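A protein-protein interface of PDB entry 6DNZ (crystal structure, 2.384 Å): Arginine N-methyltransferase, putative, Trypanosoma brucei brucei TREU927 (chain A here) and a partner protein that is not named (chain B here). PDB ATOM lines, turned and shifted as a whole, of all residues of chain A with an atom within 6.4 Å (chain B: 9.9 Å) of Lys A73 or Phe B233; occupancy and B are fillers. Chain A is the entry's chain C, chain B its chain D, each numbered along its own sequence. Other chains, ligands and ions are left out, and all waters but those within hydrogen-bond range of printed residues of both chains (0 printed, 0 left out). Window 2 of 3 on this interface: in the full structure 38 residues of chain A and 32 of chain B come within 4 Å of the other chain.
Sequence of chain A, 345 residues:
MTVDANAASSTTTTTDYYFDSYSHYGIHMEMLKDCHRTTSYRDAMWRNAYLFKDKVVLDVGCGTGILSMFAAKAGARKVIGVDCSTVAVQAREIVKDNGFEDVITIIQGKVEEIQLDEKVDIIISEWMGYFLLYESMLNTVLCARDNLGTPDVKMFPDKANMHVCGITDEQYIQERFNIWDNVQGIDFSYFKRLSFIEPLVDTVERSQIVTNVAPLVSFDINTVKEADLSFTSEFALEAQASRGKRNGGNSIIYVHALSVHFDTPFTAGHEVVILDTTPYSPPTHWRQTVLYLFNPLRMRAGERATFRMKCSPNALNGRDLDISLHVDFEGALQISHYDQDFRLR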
ATOM      1  N   TRP A  46       3.928  12.910 -22.994  1.00  0.00           N
ATOM      2  CA  TRP A  46       4.584  12.454 -21.775  1.00  0.00           C
ATOM      3  C   TRP A  46       4.789  10.947 -21.733  1.00  0.00           C
ATOM      4  O   TRP A  46       5.652  10.477 -20.985  1.00  0.00           O
ATOM      5  CB  TRP A  46       3.787  12.899 -20.549  1.00  0.00           C
ATOM      6  CG  TRP A  46       3.846  14.376 -20.322  1.00  0.00           C
ATOM      7  CD1 TRP A  46       4.365  15.313 -21.166  1.00  0.00           C
ATOM      8  CD2 TRP A  46       3.375  15.089 -19.173  1.00  0.00           C
ATOM      9  NE1 TRP A  46       4.243  16.564 -20.617  1.00  0.00           N
ATOM     10  CE2 TRP A  46       3.638  16.454 -19.393  1.00  0.00           C
ATOM     11  CE3 TRP A  46       2.758  14.705 -17.981  1.00  0.00           C
ATOM     12  CZ2 TRP A  46       3.305  17.437 -18.466  1.00  0.00           C
ATOM     13  CZ3 TRP A  46       2.426  15.682 -17.063  1.00  0.00           C
ATOM     14  CH2 TRP A  46       2.701  17.032 -17.310  1.00  0.00           C
ATOM     15  N   ALA A  49       8.095  10.885 -23.970  1.00  0.00           N
ATOM     16  CA  ALA A  49       9.043  11.944 -23.642  1.00  0.00           C
ATOM     17  C   ALA A  49      10.400  11.718 -24.290  1.00  0.00           C
ATOM     18  O   ALA A  49      11.113  12.683 -24.586  1.00  0.00           O
ATOM     19  CB  ALA A  49       9.199  12.046 -22.123  1.00  0.00           C
ATOM     20  N   LYS A  53      13.487  14.772 -26.086  1.00  0.00           N
ATOM     21  CA  LYS A  53      14.759  15.158 -25.486  1.00  0.00           C
ATOM     22  C   LYS A  53      15.647  15.861 -26.505  1.00  0.00           C
ATOM     23  O   LYS A  53      15.983  15.294 -27.549  1.00  0.00           O
ATOM     24  CB  LYS A  53      15.468  13.926 -24.925  1.00  0.00           C
ATOM     25  CG  LYS A  53      14.610  13.073 -24.001  1.00  0.00           C
ATOM     26  CD  LYS A  53      14.048  13.877 -22.836  1.00  0.00           C
ATOM     27  CE  LYS A  53      13.201  13.005 -21.921  1.00  0.00           C
ATOM     28  NZ  LYS A  53      12.617  13.786 -20.799  1.00  0.00           N
ATOM     29  N   ILE A  66      -0.757  25.864 -23.417  1.00  0.00           N
ATOM     30  CA  ILE A  66      -0.813  24.620 -22.651  1.00  0.00           C
ATOM     31  C   ILE A  66       0.035  23.536 -23.310  1.00  0.00           C
ATOM     32  O   ILE A  66       0.809  22.839 -22.645  1.00  0.00           O
ATOM     33  CB  ILE A  66      -2.276  24.172 -22.476  1.00  0.00           C
ATOM     34  CG1 ILE A  66      -2.364  22.888 -21.650  1.00  0.00           C
ATOM     35  CG2 ILE A  66      -2.949  23.975 -23.831  1.00  0.00           C
ATOM     36  CD1 ILE A  66      -1.924  23.048 -20.213  1.00  0.00           C
ATOM     37  N   SER A  68       2.534  23.825 -25.444  1.00  0.00           N
ATOM     38  CA  SER A  68       3.959  24.129 -25.422  1.00  0.00           C
ATOM     39  C   SER A  68       4.584  23.735 -24.091  1.00  0.00           C
ATOM     40  O   SER A  68       5.742  23.300 -24.049  1.00  0.00           O
ATOM     41  CB  SER A  68       4.181  25.616 -25.696  1.00  0.00           C
ATOM     42  OG  SER A  68       3.733  25.960 -26.995  1.00  0.00           O
ATOM     43  N   MET A  69       3.839  23.868 -23.003  1.00  0.00           N
ATOM     44  CA  MET A  69       4.349  23.536 -21.680  1.00  0.00           C
ATOM     45  C   MET A  69       4.377  22.028 -21.481  1.00  0.00           C
ATOM     46  O   MET A  69       5.287  21.502 -20.847  1.00  0.00           O
ATOM     47  CB  MET A  69       3.499  24.209 -20.611  1.00  0.00           C
ATOM     48  CG  MET A  69       3.201  25.658 -20.932  1.00  0.00           C
ATOM     49  SD  MET A  69       2.401  26.614 -19.453  1.00  0.00           S
ATOM     50  CE  MET A  69       4.027  27.063 -18.536  1.00  0.00           C
ATOM     51  N   PHE A  70       3.370  21.336 -22.020  1.00  0.00           N
ATOM     52  CA  PHE A  70       3.426  19.880 -22.081  1.00  0.00           C
ATOM     53  C   PHE A  70       4.705  19.425 -22.773  1.00  0.00           C
ATOM     54  O   PHE A  70       5.414  18.538 -22.285  1.00  0.00           O
ATOM     55  CB  PHE A  70       2.204  19.330 -22.823  1.00  0.00           C
ATOM     56  CG  PHE A  70       0.908  19.433 -22.055  1.00  0.00           C
ATOM     57  CD1 PHE A  70       0.891  19.502 -20.673  1.00  0.00           C
ATOM     58  CD2 PHE A  70      -0.300  19.443 -22.732  1.00  0.00           C
ATOM     59  CE1 PHE A  70      -0.302  19.589 -19.987  1.00  0.00           C
ATOM     60  CE2 PHE A  70      -1.492  19.529 -22.047  1.00  0.00           C
ATOM     61  CZ  PHE A  70      -1.493  19.602 -20.675  1.00  0.00           C
ATOM     62  N   ALA A  71       5.015  20.032 -23.921  1.00  0.00           N
ATOM     63  CA  ALA A  71       6.215  19.653 -24.657  1.00  0.00           C
ATOM     64  C   ALA A  71       7.472  19.967 -23.855  1.00  0.00           C
ATOM     65  O   ALA A  71       8.416  19.168 -23.829  1.00  0.00           O
ATOM     66  CB  ALA A  71       6.246  20.367 -26.009  1.00  0.00           C
ATOM     67  N   ALA A  72       7.504  21.123 -23.190  1.00  0.00           N
ATOM     68  CA  ALA A  72       8.663  21.469 -22.376  1.00  0.00           C
ATOM     69  C   ALA A  72       8.876  20.439 -21.272  1.00  0.00           C
ATOM     70  O   ALA A  72       9.977  19.899 -21.115  1.00  0.00           O
ATOM     71  CB  ALA A  72       8.492  22.868 -21.786  1.00  0.00           C
ATOM     72  N   LYS A  73       7.826  20.146 -20.500  1.00  0.00           N
ATOM     73  CA  LYS A  73       7.948  19.155 -19.436  1.00  0.00           C
ATOM     74  C   LYS A  73       8.354  17.794 -19.983  1.00  0.00           C
ATOM     75  O   LYS A  73       8.964  16.993 -19.264  1.00  0.00           O
ATOM     76  CB  LYS A  73       6.635  19.038 -18.660  1.00  0.00           C
ATOM     77  CG  LYS A  73       6.566  19.933 -17.429  1.00  0.00           C
ATOM     78  CD  LYS A  73       5.351  19.622 -16.562  1.00  0.00           C
ATOM     79  CE  LYS A  73       5.479  18.280 -15.845  1.00  0.00           C
ATOM     80  NZ  LYS A  73       6.633  18.237 -14.894  1.00  0.00           N
ATOM     81  N   ALA A  74       8.026  17.510 -21.244  1.00  0.00           N
ATOM     82  CA  ALA A  74       8.452  16.258 -21.855  1.00  0.00           C
ATOM     83  C   ALA A  74       9.949  16.221 -22.126  1.00  0.00           C
ATOM     84  O   ALA A  74      10.474  15.149 -22.443  1.00  0.00           O
ATOM     85  CB  ALA A  74       7.686  16.023 -23.157  1.00  0.00           C
ATOM     86  N   GLY A  75      10.642  17.353 -22.013  1.00  0.00           N
ATOM     87  CA  GLY A  75      12.081  17.401 -22.174  1.00  0.00           C
ATOM     88  C   GLY A  75      12.582  18.139 -23.398  1.00  0.00           C
ATOM     89  O   GLY A  75      13.773  18.035 -23.711  1.00  0.00           O
ATOM     90  N   ALA A  76      11.725  18.880 -24.094  1.00  0.00           N
ATOM     91  CA  ALA A  76      12.146  19.573 -25.303  1.00  0.00           C
ATOM     92  C   ALA A  76      13.199  20.626 -24.983  1.00  0.00           C
ATOM     93  O   ALA A  76      13.107  21.336 -23.978  1.00  0.00           O
ATOM     94  CB  ALA A  76      10.943  20.224 -25.983  1.00  0.00           C
ATOM     95  N   ILE A  94       2.129  33.253 -19.235  1.00  0.00           N
ATOM     96  CA  ILE A  94       1.895  31.969 -18.583  1.00  0.00           C
ATOM     97  C   ILE A  94       3.165  31.127 -18.597  1.00  0.00           C
ATOM     98  O   ILE A  94       3.572  30.568 -17.572  1.00  0.00           O
ATOM     99  CB  ILE A  94       0.726  31.235 -19.263  1.00  0.00           C
ATOM    100  CG1 ILE A  94      -0.584  31.987 -19.010  1.00  0.00           C
ATOM    101  CG2 ILE A  94       0.635  29.803 -18.761  1.00  0.00           C
ATOM    102  CD1 ILE A  94      -1.715  31.579 -19.931  1.00  0.00           C
ATOM    103  N   ASN A  98       5.525  29.829 -15.026  1.00  0.00           N
ATOM    104  CA  ASN A  98       5.843  28.457 -14.651  1.00  0.00           C
ATOM    105  C   ASN A  98       7.300  28.097 -14.914  1.00  0.00           C
ATOM    106  O   ASN A  98       7.675  26.928 -14.763  1.00  0.00           O
ATOM    107  CB  ASN A  98       4.930  27.481 -15.396  1.00  0.00           C
ATOM    108  CG  ASN A  98       3.452  27.757 -15.160  1.00  0.00           C
ATOM    109  OD1 ASN A  98       2.815  27.117 -14.325  1.00  0.00           O
ATOM    110  ND2 ASN A  98       2.900  28.711 -15.902  1.00  0.00           N
ATOM    111  N   PHE A 100       9.230  28.296 -17.792  1.00  0.00           N
ATOM    112  CA  PHE A 100       9.646  27.820 -19.104  1.00  0.00           C
ATOM    113  C   PHE A 100      10.087  28.958 -20.016  1.00  0.00           C
ATOM    114  O   PHE A 100      10.077  28.803 -21.242  1.00  0.00           O
ATOM    115  CB  PHE A 100       8.517  27.027 -19.761  1.00  0.00           C
ATOM    116  CG  PHE A 100       8.108  25.807 -18.991  1.00  0.00           C
ATOM    117  CD1 PHE A 100       8.880  24.661 -19.023  1.00  0.00           C
ATOM    118  CD2 PHE A 100       6.948  25.805 -18.241  1.00  0.00           C
ATOM    119  CE1 PHE A 100       8.503  23.536 -18.315  1.00  0.00           C
ATOM    120  CE2 PHE A 100       6.563  24.685 -17.532  1.00  0.00           C
ATOM    121  CZ  PHE A 100       7.341  23.549 -17.568  1.00  0.00           C
ATOM    122  N   GLU B 225     -11.128  31.038 -10.444  1.00  0.00           N
ATOM    123  CA  GLU B 225     -10.152  30.203  -9.765  1.00  0.00           C
ATOM    124  C   GLU B 225      -9.738  29.008 -10.608  1.00  0.00           C
ATOM    125  O   GLU B 225      -8.679  28.431 -10.352  1.00  0.00           O
ATOM    126  CB  GLU B 225     -10.695  29.728  -8.419  1.00  0.00           C
ATOM    127  CG  GLU B 225      -9.612  29.531  -7.363  1.00  0.00           C
ATOM    128  CD  GLU B 225      -8.825  30.802  -7.098  1.00  0.00           C
ATOM    129  OE1 GLU B 225      -9.436  31.893  -7.090  1.00  0.00           O
ATOM    130  OE2 GLU B 225      -7.595  30.708  -6.919  1.00  0.00           O
ATOM    131  N   PHE B 226     -10.544  28.626 -11.599  1.00  0.00           N
ATOM    132  CA  PHE B 226     -10.162  27.544 -12.498  1.00  0.00           C
ATOM    133  C   PHE B 226      -8.786  27.791 -13.099  1.00  0.00           C
ATOM    134  O   PHE B 226      -7.983  26.862 -13.243  1.00  0.00           O
ATOM    135  CB  PHE B 226     -11.212  27.397 -13.600  1.00  0.00           C
ATOM    136  CG  PHE B 226     -10.714  26.687 -14.824  1.00  0.00           C
ATOM    137  CD1 PHE B 226     -10.710  25.306 -14.887  1.00  0.00           C
ATOM    138  CD2 PHE B 226     -10.261  27.403 -15.921  1.00  0.00           C
ATOM    139  CE1 PHE B 226     -10.257  24.652 -16.014  1.00  0.00           C
ATOM    140  CE2 PHE B 226      -9.807  26.753 -17.048  1.00  0.00           C
ATOM    141  CZ  PHE B 226      -9.806  25.377 -17.096  1.00  0.00           C
ATOM    142  N   TRP B 227      -8.493  29.041 -13.455  1.00  0.00           N
ATOM    143  CA  TRP B 227      -7.205  29.380 -14.042  1.00  0.00           C
ATOM    144  C   TRP B 227      -6.075  29.337 -13.027  1.00  0.00           C
ATOM    145  O   TRP B 227      -4.909  29.446 -13.419  1.00  0.00           O
ATOM    146  CB  TRP B 227      -7.274  30.768 -14.679  1.00  0.00           C
ATOM    147  CG  TRP B 227      -8.471  30.943 -15.552  1.00  0.00           C
ATOM    148  CD1 TRP B 227      -9.662  31.497 -15.200  1.00  0.00           C
ATOM    149  CD2 TRP B 227      -8.601  30.547 -16.922  1.00  0.00           C
ATOM    150  NE1 TRP B 227     -10.526  31.477 -16.266  1.00  0.00           N
ATOM    151  CE2 TRP B 227      -9.897  30.899 -17.335  1.00  0.00           C
ATOM    152  CE3 TRP B 227      -7.748  29.933 -17.837  1.00  0.00           C
ATOM    153  CZ2 TRP B 227     -10.359  30.659 -18.624  1.00  0.00           C
ATOM    154  CZ3 TRP B 227      -8.209  29.696 -19.119  1.00  0.00           C
ATOM    155  CH2 TRP B 227      -9.502  30.057 -19.499  1.00  0.00           C
ATOM    156  N   GLY B 228      -6.390  29.187 -11.740  1.00  0.00           N
ATOM    157  CA  GLY B 228      -5.343  29.076 -10.743  1.00  0.00           C
ATOM    158  C   GLY B 228      -4.342  27.992 -11.082  1.00  0.00           C
ATOM    159  O   GLY B 228      -3.140  28.148 -10.855  1.00  0.00           O
ATOM    160  N   ASN B 229      -4.820  26.882 -11.639  1.00  0.00           N
ATOM    161  CA  ASN B 229      -3.914  25.829 -12.082  1.00  0.00           C
ATOM    162  C   ASN B 229      -4.614  24.954 -13.107  1.00  0.00           C
ATOM    163  O   ASN B 229      -5.645  24.344 -12.804  1.00  0.00           O
ATOM    164  CB  ASN B 229      -3.435  25.000 -10.908  1.00  0.00           C
ATOM    165  CG  ASN B 229      -2.037  24.476 -11.118  1.00  0.00           C
ATOM    166  OD1 ASN B 229      -1.830  23.529 -11.875  1.00  0.00           O
ATOM    167  ND2 ASN B 229      -1.066  25.083 -10.445  1.00  0.00           N
ATOM    168  N   VAL B 230      -4.037  24.870 -14.301  1.00  0.00           N
ATOM    169  CA  VAL B 230      -4.638  24.181 -15.438  1.00  0.00           C
ATOM    170  C   VAL B 230      -3.653  23.101 -15.866  1.00  0.00           C
ATOM    171  O   VAL B 230      -2.633  23.391 -16.502  1.00  0.00           O
ATOM    172  CB  VAL B 230      -4.957  25.149 -16.584  1.00  0.00           C
ATOM    173  CG1 VAL B 230      -5.477  24.404 -17.796  1.00  0.00           C
ATOM    174  CG2 VAL B 230      -5.969  26.189 -16.125  1.00  0.00           C
ATOM    175  N   TYR B 231      -3.947  21.849 -15.510  1.00  0.00           N
ATOM    176  CA  TYR B 231      -3.083  20.715 -15.840  1.00  0.00           C
ATOM    177  C   TYR B 231      -1.670  20.920 -15.299  1.00  0.00           C
ATOM    178  O   TYR B 231      -0.679  20.641 -15.977  1.00  0.00           O
ATOM    179  CB  TYR B 231      -3.052  20.465 -17.349  1.00  0.00           C
ATOM    180  CG  TYR B 231      -4.405  20.128 -17.922  1.00  0.00           C
ATOM    181  CD1 TYR B 231      -4.813  18.810 -18.063  1.00  0.00           C
ATOM    182  CD2 TYR B 231      -5.279  21.129 -18.310  1.00  0.00           C
ATOM    183  CE1 TYR B 231      -6.052  18.502 -18.581  1.00  0.00           C
ATOM    184  CE2 TYR B 231      -6.518  20.833 -18.827  1.00  0.00           C
ATOM    185  CZ  TYR B 231      -6.900  19.518 -18.959  1.00  0.00           C
ATOM    186  OH  TYR B 231      -8.137  19.223 -19.478  1.00  0.00           O
ATOM    187  N   GLY B 232      -1.576  21.410 -14.065  1.00  0.00           N
ATOM    188  CA  GLY B 232      -0.301  21.609 -13.414  1.00  0.00           C
ATOM    189  C   GLY B 232       0.308  22.984 -13.588  1.00  0.00           C
ATOM    190  O   GLY B 232       1.272  23.306 -12.882  1.00  0.00           O
ATOM    191  N   PHE B 233      -0.227  23.807 -14.483  1.00  0.00           N
ATOM    192  CA  PHE B 233       0.345  25.110 -14.790  1.00  0.00           C
ATOM    193  C   PHE B 233      -0.572  26.212 -14.284  1.00  0.00           C
ATOM    194  O   PHE B 233      -1.797  26.072 -14.301  1.00  0.00           O
ATOM    195  CB  PHE B 233       0.559  25.269 -16.296  1.00  0.00           C
ATOM    196  CG  PHE B 233       1.274  24.112 -16.925  1.00  0.00           C
ATOM    197  CD1 PHE B 233       2.634  23.940 -16.738  1.00  0.00           C
ATOM    198  CD2 PHE B 233       0.587  23.198 -17.702  1.00  0.00           C
ATOM    199  CE1 PHE B 233       3.294  22.877 -17.314  1.00  0.00           C
ATOM    200  CE2 PHE B 233       1.242  22.135 -18.281  1.00  0.00           C
ATOM    201  CZ  PHE B 233       2.597  21.974 -18.088  1.00  0.00           C
ATOM    202  N   LYS B 234       0.030  27.312 -13.837  1.00  0.00           N
ATOM    203  CA  LYS B 234      -0.719  28.456 -13.334  1.00  0.00           C
ATOM    204  C   LYS B 234      -0.997  29.421 -14.480  1.00  0.00           C
ATOM    205  O   LYS B 234      -0.062  29.913 -15.123  1.00  0.00           O
ATOM    206  CB  LYS B 234       0.053  29.158 -12.219  1.00  0.00           C
ATOM    207  CG  LYS B 234       0.318  28.284 -11.005  1.00  0.00           C
ATOM    208  CD  LYS B 234       0.714  29.116  -9.797  1.00  0.00           C
ATOM    209  CE  LYS B 234       1.035  28.241  -8.597  1.00  0.00           C
ATOM    210  NZ  LYS B 234       1.263  29.041  -7.359  1.00  0.00           N
ATOM    211  N   MET B 235      -2.275  29.695 -14.726  1.00  0.00           N
ATOM    212  CA  MET B 235      -2.676  30.596 -15.798  1.00  0.00           C
ATOM    213  C   MET B 235      -3.319  31.848 -15.217  1.00  0.00           C
ATOM    214  O   MET B 235      -4.406  32.247 -15.628  1.00  0.00           O
ATOM    215  CB  MET B 235      -3.644  29.903 -16.756  1.00  0.00           C
ATOM    216  CG  MET B 235      -3.276  28.467 -17.068  1.00  0.00           C
ATOM    217  SD  MET B 235      -3.483  28.011 -18.950  1.00  0.00           S
ATOM    218  CE  MET B 235      -5.260  28.683 -19.257  1.00  0.00           C
ATOM    219  N   GLU B 236      -2.632  32.458 -14.256  1.00  0.00           N
ATOM    220  CA  GLU B 236      -3.136  33.671 -13.621  1.00  0.00           C
ATOM    221  C   GLU B 236      -3.561  34.745 -14.617  1.00  0.00           C
ATOM    222  O   GLU B 236      -4.630  35.345 -14.415  1.00  0.00           O
ATOM    223  CB  GLU B 236      -2.063  34.225 -12.672  1.00  0.00           C
ATOM    224  CG  GLU B 236      -2.605  35.098 -11.553  1.00  0.00           C
ATOM    225  CD  GLU B 236      -3.373  34.299 -10.519  1.00  0.00           C
ATOM    226  OE1 GLU B 236      -3.364  33.053 -10.607  1.00  0.00           O
ATOM    227  OE2 GLU B 236      -3.983  34.913  -9.619  1.00  0.00           O
ATOM    228  N   PRO B 237      -2.805  35.033 -15.686  1.00  0.00           N
ATOM    229  CA  PRO B 237      -3.185  36.133 -16.586  1.00  0.00           C
ATOM    230  C   PRO B 237      -4.604  36.029 -17.119  1.00  0.00           C
ATOM    231  O   PRO B 237      -5.202  37.039 -17.501  1.00  0.00           O
ATOM    232  CB  PRO B 237      -2.158  36.024 -17.722  1.00  0.00           C
ATOM    233  CG  PRO B 237      -0.973  35.385 -17.093  1.00  0.00           C
ATOM    234  CD  PRO B 237      -1.518  34.427 -16.072  1.00  0.00           C
ATOM    235  N   MET B 238      -5.153  34.821 -17.147  1.00  0.00           N
ATOM    236  CA  MET B 238      -6.483  34.610 -17.704  1.00  0.00           C
ATOM    237  C   MET B 238      -7.572  35.116 -16.771  1.00  0.00           C
ATOM    238  O   MET B 238      -8.620  35.570 -17.229  1.00  0.00           O
ATOM    239  CB  MET B 238      -6.703  33.130 -18.000  1.00  0.00           C
ATOM    240  CG  MET B 238      -5.791  32.582 -19.079  1.00  0.00           C
ATOM    241  SD  MET B 238      -6.092  33.415 -20.813  1.00  0.00           S
ATOM    242  CE  MET B 238      -4.639  32.568 -21.791  1.00  0.00           C
ATOM    243  N   LYS B 239      -7.326  35.031 -15.461  1.00  0.00           N
ATOM    244  CA  LYS B 239      -8.315  35.490 -14.490  1.00  0.00           C
ATOM    245  C   LYS B 239      -8.808  36.890 -14.827  1.00  0.00           C
ATOM    246  O   LYS B 239     -10.011  37.167 -14.766  1.00  0.00           O
ATOM    247  CB  LYS B 239      -7.724  35.464 -13.081  1.00  0.00           C
ATOM    248  CG  LYS B 239      -7.337  34.083 -12.596  1.00  0.00           C
ATOM    249  CD  LYS B 239      -6.956  34.104 -11.125  1.00  0.00           C
ATOM    250  CE  LYS B 239      -6.483  32.741 -10.652  1.00  0.00           C
ATOM    251  NZ  LYS B 239      -6.108  32.754  -9.211  1.00  0.00           N
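OD1 of Asn A98 lies within hydrogen-bond range of N of Lys B234, at 2.8 Å.
The indole nitrogen (NE1) of Trp A46 lies within hydrogen-bond range of the backbone carbonyl oxygen (O) of Phe A70, at 2.8 Å.
The backbone carbonyl oxygen of Ile A94 sits at hydrogen-bond distance from the side-chain amide nitrogen of Asn A98 (2.6 Å).
N of Phe B233 is in hydrogen-bond range of OD1 of Asn B229 (3.1 Å).
Among the printed residues, merely in contact across the chains: Asn A98 with Phe B233, Phe A70 with Phe B233, Met A69 with Phe B233, Ile A66 with Phe B233, Ile A94 with Met B238, Ile A94 with Lys B234, Phe A100 with Phe B233, Phe A70 with Tyr B231, Ile A66 with Val B230, Ile A94 with Pro B237 and Lys A73 with Phe B233.
Of chain B, only Phe B233 (3.9 Å) comes within 4 Å of Lys A73.
Phe B233 touches just these residues of chain A: Ile A66, Met A69, Phe A70, Lys A73, Asn A98 and Phe A100.
Met A69 touches just one residue of chain B: Phe B233.
Ala A71 touches none of the printed residues of chain B.
No residue of chain B comes within 4 Å of Ala A72.
Ala A74 touches none of the printed residues of chain B.
Of the printed residues of chain B, Asn A98 touches Phe B233 and Lys B234.
Printed residues of chain B within 4 Å of Ile A94: Lys B234, Pro B237 and Met B238.
Of the printed residues of chain A, Pro B237 touches Ile A94 (3.9 Å).
Printed residues of chain A within 4 Å of Met B238: Ile A94.
The nearest residue of chain B that does not touch Lys A73 is Tyr B231 (6.1 Å).
The nearest printed residue of chain A that does not touch Tyr B231 is Ile A66 (4.02 Å).
Hydrophobic or aromatic side chains of chain A that line the printed part of chain B: Ile A66, Met A69, Phe A70, Ile A94 and Phe A100.
Printed residues of chain B that touch a printed residue of chain A: Val B230, Tyr B231, Phe B233, Lys B234, Pro B237 and Met B238.
Among the printed residues, 12 pairs touch across the chains.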
